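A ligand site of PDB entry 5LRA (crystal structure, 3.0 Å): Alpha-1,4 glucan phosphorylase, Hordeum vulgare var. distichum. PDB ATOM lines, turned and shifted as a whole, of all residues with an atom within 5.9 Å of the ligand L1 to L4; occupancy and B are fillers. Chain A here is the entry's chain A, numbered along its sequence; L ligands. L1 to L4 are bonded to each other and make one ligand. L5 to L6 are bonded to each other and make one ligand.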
ATOM      1  N   GLU A  93     -19.556   5.647   8.387  1.00  0.00           N
ATOM      2  CA  GLU A  93     -18.302   6.021   9.043  1.00  0.00           C
ATOM      3  C   GLU A  93     -17.346   6.676   8.067  1.00  0.00           C
ATOM      4  O   GLU A  93     -17.282   6.265   6.923  1.00  0.00           O
ATOM      5  CB  GLU A  93     -17.599   4.779   9.571  1.00  0.00           C
ATOM      6  CG  GLU A  93     -18.191   4.123  10.801  1.00  0.00           C
ATOM      7  CD  GLU A  93     -17.286   3.016  11.326  1.00  0.00           C
ATOM      8  OE1 GLU A  93     -16.090   3.264  11.574  1.00  0.00           O
ATOM      9  OE2 GLU A  93     -17.778   1.885  11.491  1.00  0.00           O
ATOM     10  N   ASN A 138     -15.293   5.249  13.638  1.00  0.00           N
ATOM     11  CA  ASN A 138     -15.102   4.351  14.768  1.00  0.00           C
ATOM     12  C   ASN A 138     -14.011   3.336  14.461  1.00  0.00           C
ATOM     13  O   ASN A 138     -12.949   3.365  15.072  1.00  0.00           O
ATOM     14  CB  ASN A 138     -16.440   3.660  15.079  1.00  0.00           C
ATOM     15  CG  ASN A 138     -16.383   2.734  16.288  1.00  0.00           C
ATOM     16  OD1 ASN A 138     -17.314   1.972  16.537  1.00  0.00           O
ATOM     17  ND2 ASN A 138     -15.302   2.813  17.064  1.00  0.00           N
ATOM     18  N   GLY A 139     -14.250   2.459  13.497  1.00  0.00           N
ATOM     19  CA  GLY A 139     -13.326   1.357  13.221  1.00  0.00           C
ATOM     20  C   GLY A 139     -12.778   1.334  11.808  1.00  0.00           C
ATOM     21  O   GLY A 139     -12.757   2.369  11.121  1.00  0.00           O
ATOM     22  N   GLY A 140     -12.341   0.142  11.392  1.00  0.00           N
ATOM     23  CA  GLY A 140     -11.787  -0.051  10.061  1.00  0.00           C
ATOM     24  C   GLY A 140     -12.706   0.498   8.982  1.00  0.00           C
ATOM     25  O   GLY A 140     -12.264   1.210   8.086  1.00  0.00           O
ATOM     26  N   LEU A 141     -13.991   0.183   9.094  1.00  0.00           N
ATOM     27  CA  LEU A 141     -14.986   0.585   8.104  1.00  0.00           C
ATOM     28  C   LEU A 141     -14.860   2.029   7.702  1.00  0.00           C
ATOM     29  O   LEU A 141     -15.057   2.387   6.543  1.00  0.00           O
ATOM     30  CB  LEU A 141     -16.383   0.386   8.661  1.00  0.00           C
ATOM     31  CG  LEU A 141     -17.451   0.134   7.610  1.00  0.00           C
ATOM     32  CD1 LEU A 141     -17.684  -1.356   7.489  1.00  0.00           C
ATOM     33  CD2 LEU A 141     -18.744   0.854   7.967  1.00  0.00           C
ATOM     34  N   GLY A 142     -14.560   2.877   8.697  1.00  0.00           N
ATOM     35  CA  GLY A 142     -14.465   4.311   8.511  1.00  0.00           C
ATOM     36  C   GLY A 142     -13.129   4.734   7.954  1.00  0.00           C
ATOM     37  O   GLY A 142     -13.062   5.572   7.064  1.00  0.00           O
ATOM     38  N   LEU A 170     -18.864   9.150  18.208  1.00  0.00           N
ATOM     39  CA  LEU A 170     -19.194   7.996  19.012  1.00  0.00           C
ATOM     40  C   LEU A 170     -19.008   8.350  20.490  1.00  0.00           C
ATOM     41  O   LEU A 170     -19.978   8.331  21.254  1.00  0.00           O
ATOM     42  CB  LEU A 170     -18.338   6.795  18.612  1.00  0.00           C
ATOM     43  CG  LEU A 170     -18.680   5.492  19.354  1.00  0.00           C
ATOM     44  CD1 LEU A 170     -20.063   4.979  18.956  1.00  0.00           C
ATOM     45  CD2 LEU A 170     -17.597   4.458  19.091  1.00  0.00           C
ATOM     46  N   TYR A 287     -23.671   5.400  15.508  1.00  0.00           N
ATOM     47  CA  TYR A 287     -24.143   4.116  16.026  1.00  0.00           C
ATOM     48  C   TYR A 287     -24.787   4.255  17.416  1.00  0.00           C
ATOM     49  O   TYR A 287     -24.291   3.692  18.405  1.00  0.00           O
ATOM     50  CB  TYR A 287     -22.964   3.122  16.097  1.00  0.00           C
ATOM     51  CG  TYR A 287     -22.287   2.819  14.773  1.00  0.00           C
ATOM     52  CD1 TYR A 287     -23.009   2.768  13.595  1.00  0.00           C
ATOM     53  CD2 TYR A 287     -20.930   2.551  14.721  1.00  0.00           C
ATOM     54  CE1 TYR A 287     -22.395   2.490  12.405  1.00  0.00           C
ATOM     55  CE2 TYR A 287     -20.312   2.260  13.526  1.00  0.00           C
ATOM     56  CZ  TYR A 287     -21.050   2.230  12.363  1.00  0.00           C
ATOM     57  OH  TYR A 287     -20.478   1.955  11.144  1.00  0.00           O
ATOM     58  N   ASP A 290     -29.349   1.098  20.643  1.00  0.00           N
ATOM     59  CA  ASP A 290     -30.595   0.695  20.008  1.00  0.00           C
ATOM     60  C   ASP A 290     -31.304  -0.475  20.683  1.00  0.00           C
ATOM     61  O   ASP A 290     -32.085  -1.180  20.046  1.00  0.00           O
ATOM     62  CB  ASP A 290     -30.323   0.326  18.538  1.00  0.00           C
ATOM     63  CG  ASP A 290     -29.435  -0.918  18.401  1.00  0.00           C
ATOM     64  OD1 ASP A 290     -28.880  -1.387  19.428  1.00  0.00           O
ATOM     65  OD2 ASP A 290     -29.282  -1.417  17.259  1.00  0.00           O
ATOM     66  N   GLU A 291     -31.044  -0.693  21.974  1.00  0.00           N
ATOM     67  CA  GLU A 291     -31.792  -1.690  22.720  1.00  0.00           C
ATOM     68  C   GLU A 291     -33.211  -1.205  22.989  1.00  0.00           C
ATOM     69  O   GLU A 291     -34.033  -1.945  23.503  1.00  0.00           O
ATOM     70  CB  GLU A 291     -31.096  -2.010  24.045  1.00  0.00           C
ATOM     71  CG  GLU A 291     -29.903  -2.930  23.880  1.00  0.00           C
ATOM     72  CD  GLU A 291     -28.983  -2.926  25.098  1.00  0.00           C
ATOM     73  OE1 GLU A 291     -27.803  -3.306  24.942  1.00  0.00           O
ATOM     74  OE2 GLU A 291     -29.439  -2.553  26.201  1.00  0.00           O
ATOM     75  N   ARG A 299     -31.704   4.946  14.530  1.00  0.00           N
ATOM     76  CA  ARG A 299     -30.689   4.224  13.776  1.00  0.00           C
ATOM     77  C   ARG A 299     -31.148   4.112  12.324  1.00  0.00           C
ATOM     78  O   ARG A 299     -30.359   4.250  11.405  1.00  0.00           O
ATOM     79  CB  ARG A 299     -30.504   2.823  14.386  1.00  0.00           C
ATOM     80  CG  ARG A 299     -29.225   2.106  14.031  1.00  0.00           C
ATOM     81  CD  ARG A 299     -28.051   2.663  14.805  1.00  0.00           C
ATOM     82  NE  ARG A 299     -27.691   1.882  15.998  1.00  0.00           N
ATOM     83  CZ  ARG A 299     -26.679   0.999  16.099  1.00  0.00           C
ATOM     84  NH1 ARG A 299     -25.902   0.733  15.058  1.00  0.00           N
ATOM     85  NH2 ARG A 299     -26.429   0.381  17.238  1.00  0.00           N
ATOM     86  N   ASP A 341     -21.158  -2.075   3.774  1.00  0.00           N
ATOM     87  CA  ASP A 341     -21.977  -2.855   4.726  1.00  0.00           C
ATOM     88  C   ASP A 341     -23.470  -2.615   4.529  1.00  0.00           C
ATOM     89  O   ASP A 341     -23.854  -1.991   3.547  1.00  0.00           O
ATOM     90  CB  ASP A 341     -21.540  -2.619   6.165  1.00  0.00           C
ATOM     91  CG  ASP A 341     -21.530  -3.911   6.982  1.00  0.00           C
ATOM     92  OD1 ASP A 341     -22.605  -4.523   7.093  1.00  0.00           O
ATOM     93  OD2 ASP A 341     -20.452  -4.301   7.474  1.00  0.00           O
ATOM     94  N   HIS A 343     -25.761  -0.842   6.161  1.00  0.00           N
ATOM     95  CA  HIS A 343     -26.397   0.397   6.605  1.00  0.00           C
ATOM     96  C   HIS A 343     -27.119   1.136   5.456  1.00  0.00           C
ATOM     97  O   HIS A 343     -28.267   1.560   5.632  1.00  0.00           O
ATOM     98  CB  HIS A 343     -25.394   1.311   7.319  1.00  0.00           C
ATOM     99  CG  HIS A 343     -24.597   0.621   8.405  1.00  0.00           C
ATOM    100  ND1 HIS A 343     -23.249   0.355   8.275  1.00  0.00           N
ATOM    101  CD2 HIS A 343     -24.966   0.161   9.617  1.00  0.00           C
ATOM    102  CE1 HIS A 343     -22.821  -0.243   9.380  1.00  0.00           C
ATOM    103  NE2 HIS A 343     -23.845  -0.368  10.206  1.00  0.00           N
ATOM    104  N   HIS A 379     -18.508  -6.514   5.249  1.00  0.00           N
ATOM    105  CA  HIS A 379     -17.288  -6.301   6.031  1.00  0.00           C
ATOM    106  C   HIS A 379     -17.102  -7.162   7.253  1.00  0.00           C
ATOM    107  O   HIS A 379     -16.040  -7.133   7.863  1.00  0.00           O
ATOM    108  CB  HIS A 379     -17.240  -4.861   6.502  1.00  0.00           C
ATOM    109  CG  HIS A 379     -17.068  -3.895   5.385  1.00  0.00           C
ATOM    110  ND1 HIS A 379     -15.825  -3.455   4.975  1.00  0.00           N
ATOM    111  CD2 HIS A 379     -17.966  -3.313   4.563  1.00  0.00           C
ATOM    112  CE1 HIS A 379     -15.972  -2.625   3.965  1.00  0.00           C
ATOM    113  NE2 HIS A 379     -17.267  -2.528   3.698  1.00  0.00           N
ATOM    114  N   THR A 380     -18.129  -7.895   7.654  1.00  0.00           N
ATOM    115  CA  THR A 380     -17.982  -8.817   8.765  1.00  0.00           C
ATOM    116  C   THR A 380     -19.140  -9.780   8.799  1.00  0.00           C
ATOM    117  O   THR A 380     -20.312  -9.387   8.732  1.00  0.00           O
ATOM    118  CB  THR A 380     -17.822  -8.143  10.168  1.00  0.00           C
ATOM    119  OG1 THR A 380     -18.080  -6.730  10.086  1.00  0.00           O
ATOM    120  CG2 THR A 380     -16.407  -8.386  10.737  1.00  0.00           C
ATOM    121  N   LEU A 382     -19.910 -10.914  11.431  1.00  0.00           N
ATOM    122  CA  LEU A 382     -20.551 -10.536  12.735  1.00  0.00           C
ATOM    123  C   LEU A 382     -21.989  -9.967  12.600  1.00  0.00           C
ATOM    124  O   LEU A 382     -22.218  -9.071  11.787  1.00  0.00           O
ATOM    125  CB  LEU A 382     -19.691  -9.501  13.479  1.00  0.00           C
ATOM    126  CG  LEU A 382     -18.642  -9.912  14.525  1.00  0.00           C
ATOM    127  CD1 LEU A 382     -19.286 -10.672  15.682  1.00  0.00           C
ATOM    128  CD2 LEU A 382     -17.501 -10.722  13.919  1.00  0.00           C
ATOM    129  N   GLU A 384     -24.078  -7.944  14.179  1.00  0.00           N
ATOM    130  CA  GLU A 384     -24.400  -6.525  14.390  1.00  0.00           C
ATOM    131  C   GLU A 384     -24.363  -5.772  13.052  1.00  0.00           C
ATOM    132  O   GLU A 384     -24.894  -4.653  12.923  1.00  0.00           O
ATOM    133  CB  GLU A 384     -23.383  -5.899  15.344  1.00  0.00           C
ATOM    134  CG  GLU A 384     -23.027  -6.747  16.567  1.00  0.00           C
ATOM    135  CD  GLU A 384     -21.539  -7.044  16.680  1.00  0.00           C
ATOM    136  OE1 GLU A 384     -20.688  -6.248  16.192  1.00  0.00           O
ATOM    137  OE2 GLU A 384     -21.198  -8.094  17.263  1.00  0.00           O
ATOM    138  N   ALA A 385     -23.704  -6.388  12.050  1.00  0.00           N
ATOM    139  CA  ALA A 385     -23.622  -5.877  10.680  1.00  0.00           C
ATOM    140  C   ALA A 385     -24.673  -6.526   9.755  1.00  0.00           C
ATOM    141  O   ALA A 385     -25.100  -5.877   8.794  1.00  0.00           O
ATOM    142  CB  ALA A 385     -22.222  -6.099  10.128  1.00  0.00           C
ATOM    143  N   ARG A 657     -10.616  -1.825  18.437  1.00  0.00           N
ATOM    144  CA  ARG A 657     -11.916  -1.883  19.114  1.00  0.00           C
ATOM    145  C   ARG A 657     -11.936  -3.022  20.136  1.00  0.00           C
ATOM    146  O   ARG A 657     -11.515  -4.134  19.832  1.00  0.00           O
ATOM    147  CB  ARG A 657     -13.064  -2.023  18.092  1.00  0.00           C
ATOM    148  CG  ARG A 657     -13.042  -0.998  16.949  1.00  0.00           C
ATOM    149  CD  ARG A 657     -14.355  -0.947  16.158  1.00  0.00           C
ATOM    150  NE  ARG A 657     -14.653  -2.191  15.426  1.00  0.00           N
ATOM    151  CZ  ARG A 657     -15.448  -3.180  15.865  1.00  0.00           C
ATOM    152  NH1 ARG A 657     -15.640  -4.254  15.096  1.00  0.00           N
ATOM    153  NH2 ARG A 657     -16.066  -3.113  17.040  1.00  0.00           N
ATOM    154  N   ILE A 658     -12.416  -2.749  21.339  1.00  0.00           N
ATOM    155  CA  ILE A 658     -12.317  -3.694  22.445  1.00  0.00           C
ATOM    156  C   ILE A 658     -13.474  -4.692  22.401  1.00  0.00           C
ATOM    157  O   ILE A 658     -14.598  -4.368  22.769  1.00  0.00           O
ATOM    158  CB  ILE A 658     -12.319  -2.977  23.813  1.00  0.00           C
ATOM    159  CG1 ILE A 658     -11.221  -1.912  23.875  1.00  0.00           C
ATOM    160  CG2 ILE A 658     -12.164  -3.986  24.951  1.00  0.00           C
ATOM    161  CD1 ILE A 658      -9.805  -2.448  23.701  1.00  0.00           C
ATOM    162  N   HIS A 659     -13.187  -5.896  21.937  1.00  0.00           N
ATOM    163  CA  HIS A 659     -14.224  -6.879  21.683  1.00  0.00           C
ATOM    164  C   HIS A 659     -13.730  -8.204  22.213  1.00  0.00           C
ATOM    165  O   HIS A 659     -12.532  -8.506  22.120  1.00  0.00           O
ATOM    166  CB  HIS A 659     -14.486  -6.963  20.172  1.00  0.00           C
ATOM    167  CG  HIS A 659     -15.897  -7.266  19.801  1.00  0.00           C
ATOM    168  ND1 HIS A 659     -16.555  -8.416  20.206  1.00  0.00           N
ATOM    169  CD2 HIS A 659     -16.782  -6.596  19.010  1.00  0.00           C
ATOM    170  CE1 HIS A 659     -17.774  -8.422  19.706  1.00  0.00           C
ATOM    171  NE2 HIS A 659     -17.941  -7.330  18.980  1.00  0.00           N
ATOM    172  N   GLU A 660     -14.635  -9.001  22.758  1.00  0.00           N
ATOM    173  CA  GLU A 660     -14.275 -10.324  23.237  1.00  0.00           C
ATOM    174  C   GLU A 660     -13.519 -11.082  22.133  1.00  0.00           C
ATOM    175  O   GLU A 660     -12.556 -11.786  22.437  1.00  0.00           O
ATOM    176  CB  GLU A 660     -15.526 -11.094  23.674  1.00  0.00           C
ATOM    177  CG  GLU A 660     -16.162 -10.577  24.971  1.00  0.00           C
ATOM    178  CD  GLU A 660     -17.507 -11.226  25.290  1.00  0.00           C
ATOM    179  OE1 GLU A 660     -18.397 -11.245  24.405  1.00  0.00           O
ATOM    180  OE2 GLU A 660     -17.679 -11.694  26.432  1.00  0.00           O
ATOM    181  N   TYR A 661     -13.943 -10.898  20.883  1.00  0.00           N
ATOM    182  CA  TYR A 661     -13.408 -11.676  19.747  1.00  0.00           C
ATOM    183  C   TYR A 661     -12.042 -11.224  19.249  1.00  0.00           C
ATOM    184  O   TYR A 661     -11.311 -12.018  18.657  1.00  0.00           O
ATOM    185  CB  TYR A 661     -14.430 -11.703  18.581  1.00  0.00           C
ATOM    186  CG  TYR A 661     -14.260 -10.685  17.450  1.00  0.00           C
ATOM    187  CD1 TYR A 661     -13.348 -10.882  16.415  1.00  0.00           C
ATOM    188  CD2 TYR A 661     -15.081  -9.551  17.389  1.00  0.00           C
ATOM    189  CE1 TYR A 661     -13.219  -9.968  15.380  1.00  0.00           C
ATOM    190  CE2 TYR A 661     -14.951  -8.638  16.354  1.00  0.00           C
ATOM    191  CZ  TYR A 661     -14.027  -8.851  15.355  1.00  0.00           C
ATOM    192  OH  TYR A 661     -13.901  -7.947  14.342  1.00  0.00           O
ATOM    193  N   PHE A 702     -17.441  -0.450  23.131  1.00  0.00           N
ATOM    194  CA  PHE A 702     -18.802   0.057  22.915  1.00  0.00           C
ATOM    195  C   PHE A 702     -19.451   0.183  24.290  1.00  0.00           C
ATOM    196  O   PHE A 702     -19.376  -0.732  25.115  1.00  0.00           O
ATOM    197  CB  PHE A 702     -19.627  -0.830  21.949  1.00  0.00           C
ATOM    198  CG  PHE A 702     -20.868  -0.146  21.408  1.00  0.00           C
ATOM    199  CD1 PHE A 702     -20.790   0.735  20.322  1.00  0.00           C
ATOM    200  CD2 PHE A 702     -22.124  -0.393  21.971  1.00  0.00           C
ATOM    201  CE1 PHE A 702     -21.926   1.367  19.828  1.00  0.00           C
ATOM    202  CE2 PHE A 702     -23.270   0.228  21.475  1.00  0.00           C
ATOM    203  CZ  PHE A 702     -23.169   1.108  20.397  1.00  0.00           C
ATOM    204  N   THR A 704     -22.217   0.260  25.874  1.00  0.00           N
ATOM    205  CA  THR A 704     -23.269  -0.588  26.415  1.00  0.00           C
ATOM    206  C   THR A 704     -22.784  -2.047  26.606  1.00  0.00           C
ATOM    207  O   THR A 704     -23.309  -2.799  27.441  1.00  0.00           O
ATOM    208  CB  THR A 704     -24.529  -0.460  25.505  1.00  0.00           C
ATOM    209  OG1 THR A 704     -25.715  -0.636  26.292  1.00  0.00           O
ATOM    210  CG2 THR A 704     -24.506  -1.435  24.323  1.00  0.00           C
ATOM    211  N   TYR A 705     -21.738  -2.417  25.851  1.00  0.00           N
ATOM    212  CA  TYR A 705     -21.058  -3.713  25.914  1.00  0.00           C
ATOM    213  C   TYR A 705     -20.370  -3.890  27.272  1.00  0.00           C
ATOM    214  O   TYR A 705     -19.214  -3.494  27.467  1.00  0.00           O
ATOM    215  CB  TYR A 705     -20.026  -3.787  24.769  1.00  0.00           C
ATOM    216  CG  TYR A 705     -19.534  -5.153  24.315  1.00  0.00           C
ATOM    217  CD1 TYR A 705     -19.558  -6.269  25.162  1.00  0.00           C
ATOM    218  CD2 TYR A 705     -18.984  -5.306  23.046  1.00  0.00           C
ATOM    219  CE1 TYR A 705     -19.074  -7.492  24.741  1.00  0.00           C
ATOM    220  CE2 TYR A 705     -18.497  -6.530  22.612  1.00  0.00           C
ATOM    221  CZ  TYR A 705     -18.552  -7.618  23.459  1.00  0.00           C
ATOM    222  OH  TYR A 705     -18.078  -8.851  23.037  1.00  0.00           O
ATOM    223  N   VAL A 706     -21.096  -4.503  28.206  1.00  0.00           N
ATOM    224  CA  VAL A 706     -20.666  -4.601  29.598  1.00  0.00           C
ATOM    225  C   VAL A 706     -19.354  -5.332  29.772  1.00  0.00           C
ATOM    226  O   VAL A 706     -18.484  -4.865  30.517  1.00  0.00           O
ATOM    227  CB  VAL A 706     -21.717  -5.333  30.456  1.00  0.00           C
ATOM    228  CG1 VAL A 706     -21.188  -5.543  31.878  1.00  0.00           C
ATOM    229  CG2 VAL A 706     -23.035  -4.567  30.441  1.00  0.00           C
ATOM    230  N   TYR A 858     -24.775 -18.783  27.216  1.00  0.00           N
ATOM    231  CA  TYR A 858     -24.440 -17.457  26.709  1.00  0.00           C
ATOM    232  C   TYR A 858     -23.526 -16.694  27.666  1.00  0.00           C
ATOM    233  O   TYR A 858     -23.782 -16.673  28.867  1.00  0.00           O
ATOM    234  CB  TYR A 858     -25.721 -16.629  26.475  1.00  0.00           C
ATOM    235  CG  TYR A 858     -25.468 -15.330  25.765  1.00  0.00           C
ATOM    236  CD1 TYR A 858     -25.511 -15.247  24.380  1.00  0.00           C
ATOM    237  CD2 TYR A 858     -25.150 -14.177  26.483  1.00  0.00           C
ATOM    238  CE1 TYR A 858     -25.257 -14.061  23.720  1.00  0.00           C
ATOM    239  CE2 TYR A 858     -24.884 -12.974  25.833  1.00  0.00           C
ATOM    240  CZ  TYR A 858     -24.939 -12.930  24.457  1.00  0.00           C
ATOM    241  OH  TYR A 858     -24.682 -11.749  23.813  1.00  0.00           O
ATOM    242  N   PHE A 864     -14.809 -17.667  22.516  1.00  0.00           N
ATOM    243  CA  PHE A 864     -13.755 -17.171  21.634  1.00  0.00           C
ATOM    244  C   PHE A 864     -12.406 -17.871  21.823  1.00  0.00           C
ATOM    245  O   PHE A 864     -11.374 -17.346  21.388  1.00  0.00           O
ATOM    246  CB  PHE A 864     -13.630 -15.681  21.803  1.00  0.00           C
ATOM    247  CG  PHE A 864     -14.889 -14.955  21.498  1.00  0.00           C
ATOM    248  CD1 PHE A 864     -15.192 -14.586  20.205  1.00  0.00           C
ATOM    249  CD2 PHE A 864     -15.795 -14.674  22.502  1.00  0.00           C
ATOM    250  CE1 PHE A 864     -16.369 -13.916  19.918  1.00  0.00           C
ATOM    251  CE2 PHE A 864     -16.969 -13.999  22.223  1.00  0.00           C
ATOM    252  CZ  PHE A 864     -17.259 -13.620  20.919  1.00  0.00           C
HETATM  253  C1  LIG L   1     -23.637  -7.694  23.934  1.00  0.00           C
HETATM  254  C2  LIG L   1     -23.708  -6.599  22.857  1.00  0.00           C
HETATM  255  C3  LIG L   1     -22.507  -6.647  21.914  1.00  0.00           C
HETATM  256  C4  LIG L   1     -22.277  -8.095  21.452  1.00  0.00           C
HETATM  257  C5  LIG L   1     -21.118  -8.221  20.467  1.00  0.00           C
HETATM  258  C6  LIG L   1     -23.149  -9.046  23.417  1.00  0.00           C
HETATM  259  O1  LIG L   1     -22.814  -9.902  24.507  1.00  0.00           O
HETATM  260  O2  LIG L   1     -24.921  -7.854  24.515  1.00  0.00           O
HETATM  261  O3  LIG L   1     -23.799  -5.361  23.508  1.00  0.00           O
HETATM  262  O4  LIG L   1     -22.659  -5.784  20.786  1.00  0.00           O
HETATM  263  O5  LIG L   1     -22.012  -8.896  22.587  1.00  0.00           O
HETATM  264  O6  LIG L   1     -20.821  -9.572  20.195  1.00  0.00           O
HETATM  265  C1  LG2 L   2     -22.360  -4.386  21.052  1.00  0.00           C
HETATM  266  C2  LG2 L   2     -23.555  -3.484  20.717  1.00  0.00           C
HETATM  267  C3  LG2 L   2     -23.704  -3.250  19.206  1.00  0.00           C
HETATM  268  C4  LG2 L   2     -22.388  -2.733  18.631  1.00  0.00           C
HETATM  269  C5  LG2 L   2     -21.245  -3.678  18.992  1.00  0.00           C
HETATM  270  C6  LG2 L   2     -19.927  -3.122  18.465  1.00  0.00           C
HETATM  271  O1  LG2 L   2     -24.727  -4.015  21.295  1.00  0.00           O
HETATM  272  O2  LG2 L   2     -24.752  -2.355  18.882  1.00  0.00           O
HETATM  273  O3  LG2 L   2     -22.446  -2.651  17.212  1.00  0.00           O
HETATM  274  O4  LG2 L   2     -21.185  -3.920  20.392  1.00  0.00           O
HETATM  275  O5  LG2 L   2     -18.840  -3.401  19.314  1.00  0.00           O
HETATM  276  C1  LG3 L   3     -22.237  -1.326  16.694  1.00  0.00           C
HETATM  277  C2  LG3 L   3     -22.929  -1.288  15.343  1.00  0.00           C
HETATM  278  C3  LG3 L   3     -22.137  -2.074  14.329  1.00  0.00           C
HETATM  279  C4  LG3 L   3     -20.796  -1.372  14.168  1.00  0.00           C
HETATM  280  C5  LG3 L   3     -20.081  -1.402  15.518  1.00  0.00           C
HETATM  281  C6  LG3 L   3     -18.811  -0.551  15.511  1.00  0.00           C
HETATM  282  O1  LG3 L   3     -24.194  -1.877  15.509  1.00  0.00           O
HETATM  283  O2  LG3 L   3     -22.820  -2.151  13.107  1.00  0.00           O
HETATM  284  O3  LG3 L   3     -20.039  -2.113  13.235  1.00  0.00           O
HETATM  285  O4  LG3 L   3     -20.880  -0.943  16.597  1.00  0.00           O
HETATM  286  O5  LG3 L   3     -18.284  -0.523  16.823  1.00  0.00           O
HETATM  287  C1  LG4 L   4     -19.598  -1.385  12.076  1.00  0.00           C
HETATM  288  C2  LG4 L   4     -19.663  -2.326  10.869  1.00  0.00           C
HETATM  289  C3  LG4 L   4     -18.566  -3.377  10.905  1.00  0.00           C
HETATM  290  C4  LG4 L   4     -17.196  -2.715  11.056  1.00  0.00           C
HETATM  291  C5  LG4 L   4     -17.218  -1.784  12.273  1.00  0.00           C
HETATM  292  C6  LG4 L   4     -15.884  -1.044  12.479  1.00  0.00           C
HETATM  293  O1  LG4 L   4     -20.932  -2.975  10.846  1.00  0.00           O
HETATM  294  O2  LG4 L   4     -18.630  -4.186   9.750  1.00  0.00           O
HETATM  295  O3  LG4 L   4     -16.202  -3.721  11.195  1.00  0.00           O
HETATM  296  O4  LG4 L   4     -18.287  -0.850  12.216  1.00  0.00           O
HETATM  297  O5  LG4 L   4     -15.839   0.200  11.828  1.00  0.00           O
HETATM  298  C1  LG5 L   5     -26.057 -19.382  21.469  1.00  0.00           C
HETATM  299  C2  LG5 L   5     -25.080 -19.790  22.589  1.00  0.00           C
HETATM  300  C3  LG5 L   5     -24.016 -18.707  22.832  1.00  0.00           C
HETATM  301  C4  LG5 L   5     -23.485 -18.010  21.563  1.00  0.00           C
HETATM  302  C5  LG5 L   5     -24.402 -18.148  20.347  1.00  0.00           C
HETATM  303  C6  LG5 L   5     -23.593 -18.145  19.053  1.00  0.00           C
HETATM  304  O1  LG5 L   5     -26.845 -18.443  22.175  1.00  0.00           O
HETATM  305  O2  LG5 L   5     -25.779 -20.101  23.788  1.00  0.00           O
HETATM  306  O3  LG5 L   5     -22.906 -19.305  23.493  1.00  0.00           O
HETATM  307  O4  LG5 L   5     -23.317 -16.626  21.803  1.00  0.00           O
HETATM  308  O5  LG5 L   5     -25.143 -19.365  20.396  1.00  0.00           O
HETATM  309  O6  LG5 L   5     -24.464 -18.516  18.021  1.00  0.00           O
HETATM  310  C1  LG6 L   6     -21.930 -16.230  21.699  1.00  0.00           C
HETATM  311  C2  LG6 L   6     -21.206 -16.364  23.064  1.00  0.00           C
HETATM  312  C3  LG6 L   6     -21.044 -15.073  23.881  1.00  0.00           C
HETATM  313  C4  LG6 L   6     -20.732 -13.894  22.971  1.00  0.00           C
HETATM  314  C5  LG6 L   6     -21.780 -13.785  21.863  1.00  0.00           C
HETATM  315  C6  LG6 L   6     -21.538 -12.575  20.950  1.00  0.00           C
HETATM  316  O1  LG6 L   6     -21.800 -17.340  23.903  1.00  0.00           O
HETATM  317  O2  LG6 L   6     -20.041 -15.236  24.875  1.00  0.00           O
HETATM  318  O3  LG6 L   6     -20.674 -12.703  23.743  1.00  0.00           O
HETATM  319  O4  LG6 L   6     -21.788 -14.962  21.076  1.00  0.00           O
HETATM  320  O5  LG6 L   6     -20.779 -11.553  21.566  1.00  0.00           O
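An oxygen (O6) of LIG L1 lies within hydrogen-bond range of an oxygen (O5) of LG6 L6, at 2.4 Å.
The backbone NH of Asn 138 sits at hydrogen-bond distance from the side-chain carboxylate of Glu 93 (3.0 Å). OE1 of Glu 93 is in hydrogen-bond range of N of Gly 139 (2.8 Å). The side-chain hydroxyl of Tyr 287 lies within hydrogen-bond range of the side-chain carboxylate of Glu 93. N of Gly 142 lies within hydrogen-bond range of OE1 of Glu 93, at 3.3 Å. NH2 of Arg 299 is in salt-bridge range of OD2 of Asp 290 (3.4 Å). ND1 of His 659 sits at hydrogen-bond distance from OH of Tyr 705 (3.2 Å). OH of Tyr 705 lies within hydrogen-bond range of OE1 of Glu 660 (2.8 Å).
An oxygen (O5) of LG4 L4 is in hydrogen-bond range of the side-chain carboxylate of Glu 93. The side-chain hydroxyl (OG1) of Thr 380 lies within hydrogen-bond range of an oxygen (O2) of LG4 L4, 2.6 Å away. The side-chain amide oxygen (OD1) of Asn 138 lies within hydrogen-bond range of an oxygen (O5) of LG3 L3, 2.7 Å away. OH of Tyr 858 sits at hydrogen-bond distance from O1 of LIG L1 (2.7 Å). OD2 of Asp 341 sits at hydrogen-bond distance from O2 of LG4 L4, at 2.9 Å. N of Gly 139 lies close to O5 of LG4 L4 (3.2 Å). NH1 of Arg 299 lies within hydrogen-bond range of O1 of LG3 L3 (3.2 Å). An oxygen (O2) of LG3 L3 is in hydrogen-bond range of the backbone carbonyl oxygen (O) of Glu 384 (3.3 Å). An oxygen (O6) of LIG L1 lies close to the side-chain carboxylate of Glu 384 (3.3 Å). The backbone NH (N) of Leu 141 lies close to an oxygen (O5) of LG4 L4, 3.3 Å away. NH2 of Arg 657 lies within hydrogen-bond range of O5 of LG3 L3. The side-chain carboxylate of Glu 660 is in hydrogen-bond range of an oxygen (O3) of LG6 L6, 2.8 Å away.
Gly 140 touches the ligand L1 to L4. OH of Tyr 287 touches C1 of LG4 L4 (3.6 Å). NE2 of His 343 touches O2 of LG3 L3, at 3.6 Å. His 379 touches the ligand L1 to L4. CB of Ala 385 touches O1 of LG4 L4, 3.5 Å away. CE1 of His 659 touches O6 of LIG L1, 3.3 Å away. CD2 of Phe 702 touches C2 of LG2 L2, at 3.6 Å. CG2 of Thr 704 touches O1 of LG2 L2, at 3.98 Å. Tyr 705 touches the ligand L1 to L4. Hydrophobic or aromatic side chains within 4 Å of the ligand L1 to L4: Leu 141, Tyr 287, His 343, His 379, Ala 385, His 659, Phe 702, Tyr 705 and Tyr 858. The nearest printed residue that does not touch the ligand L1 to L4 is Asp 290 (4.3 Å).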
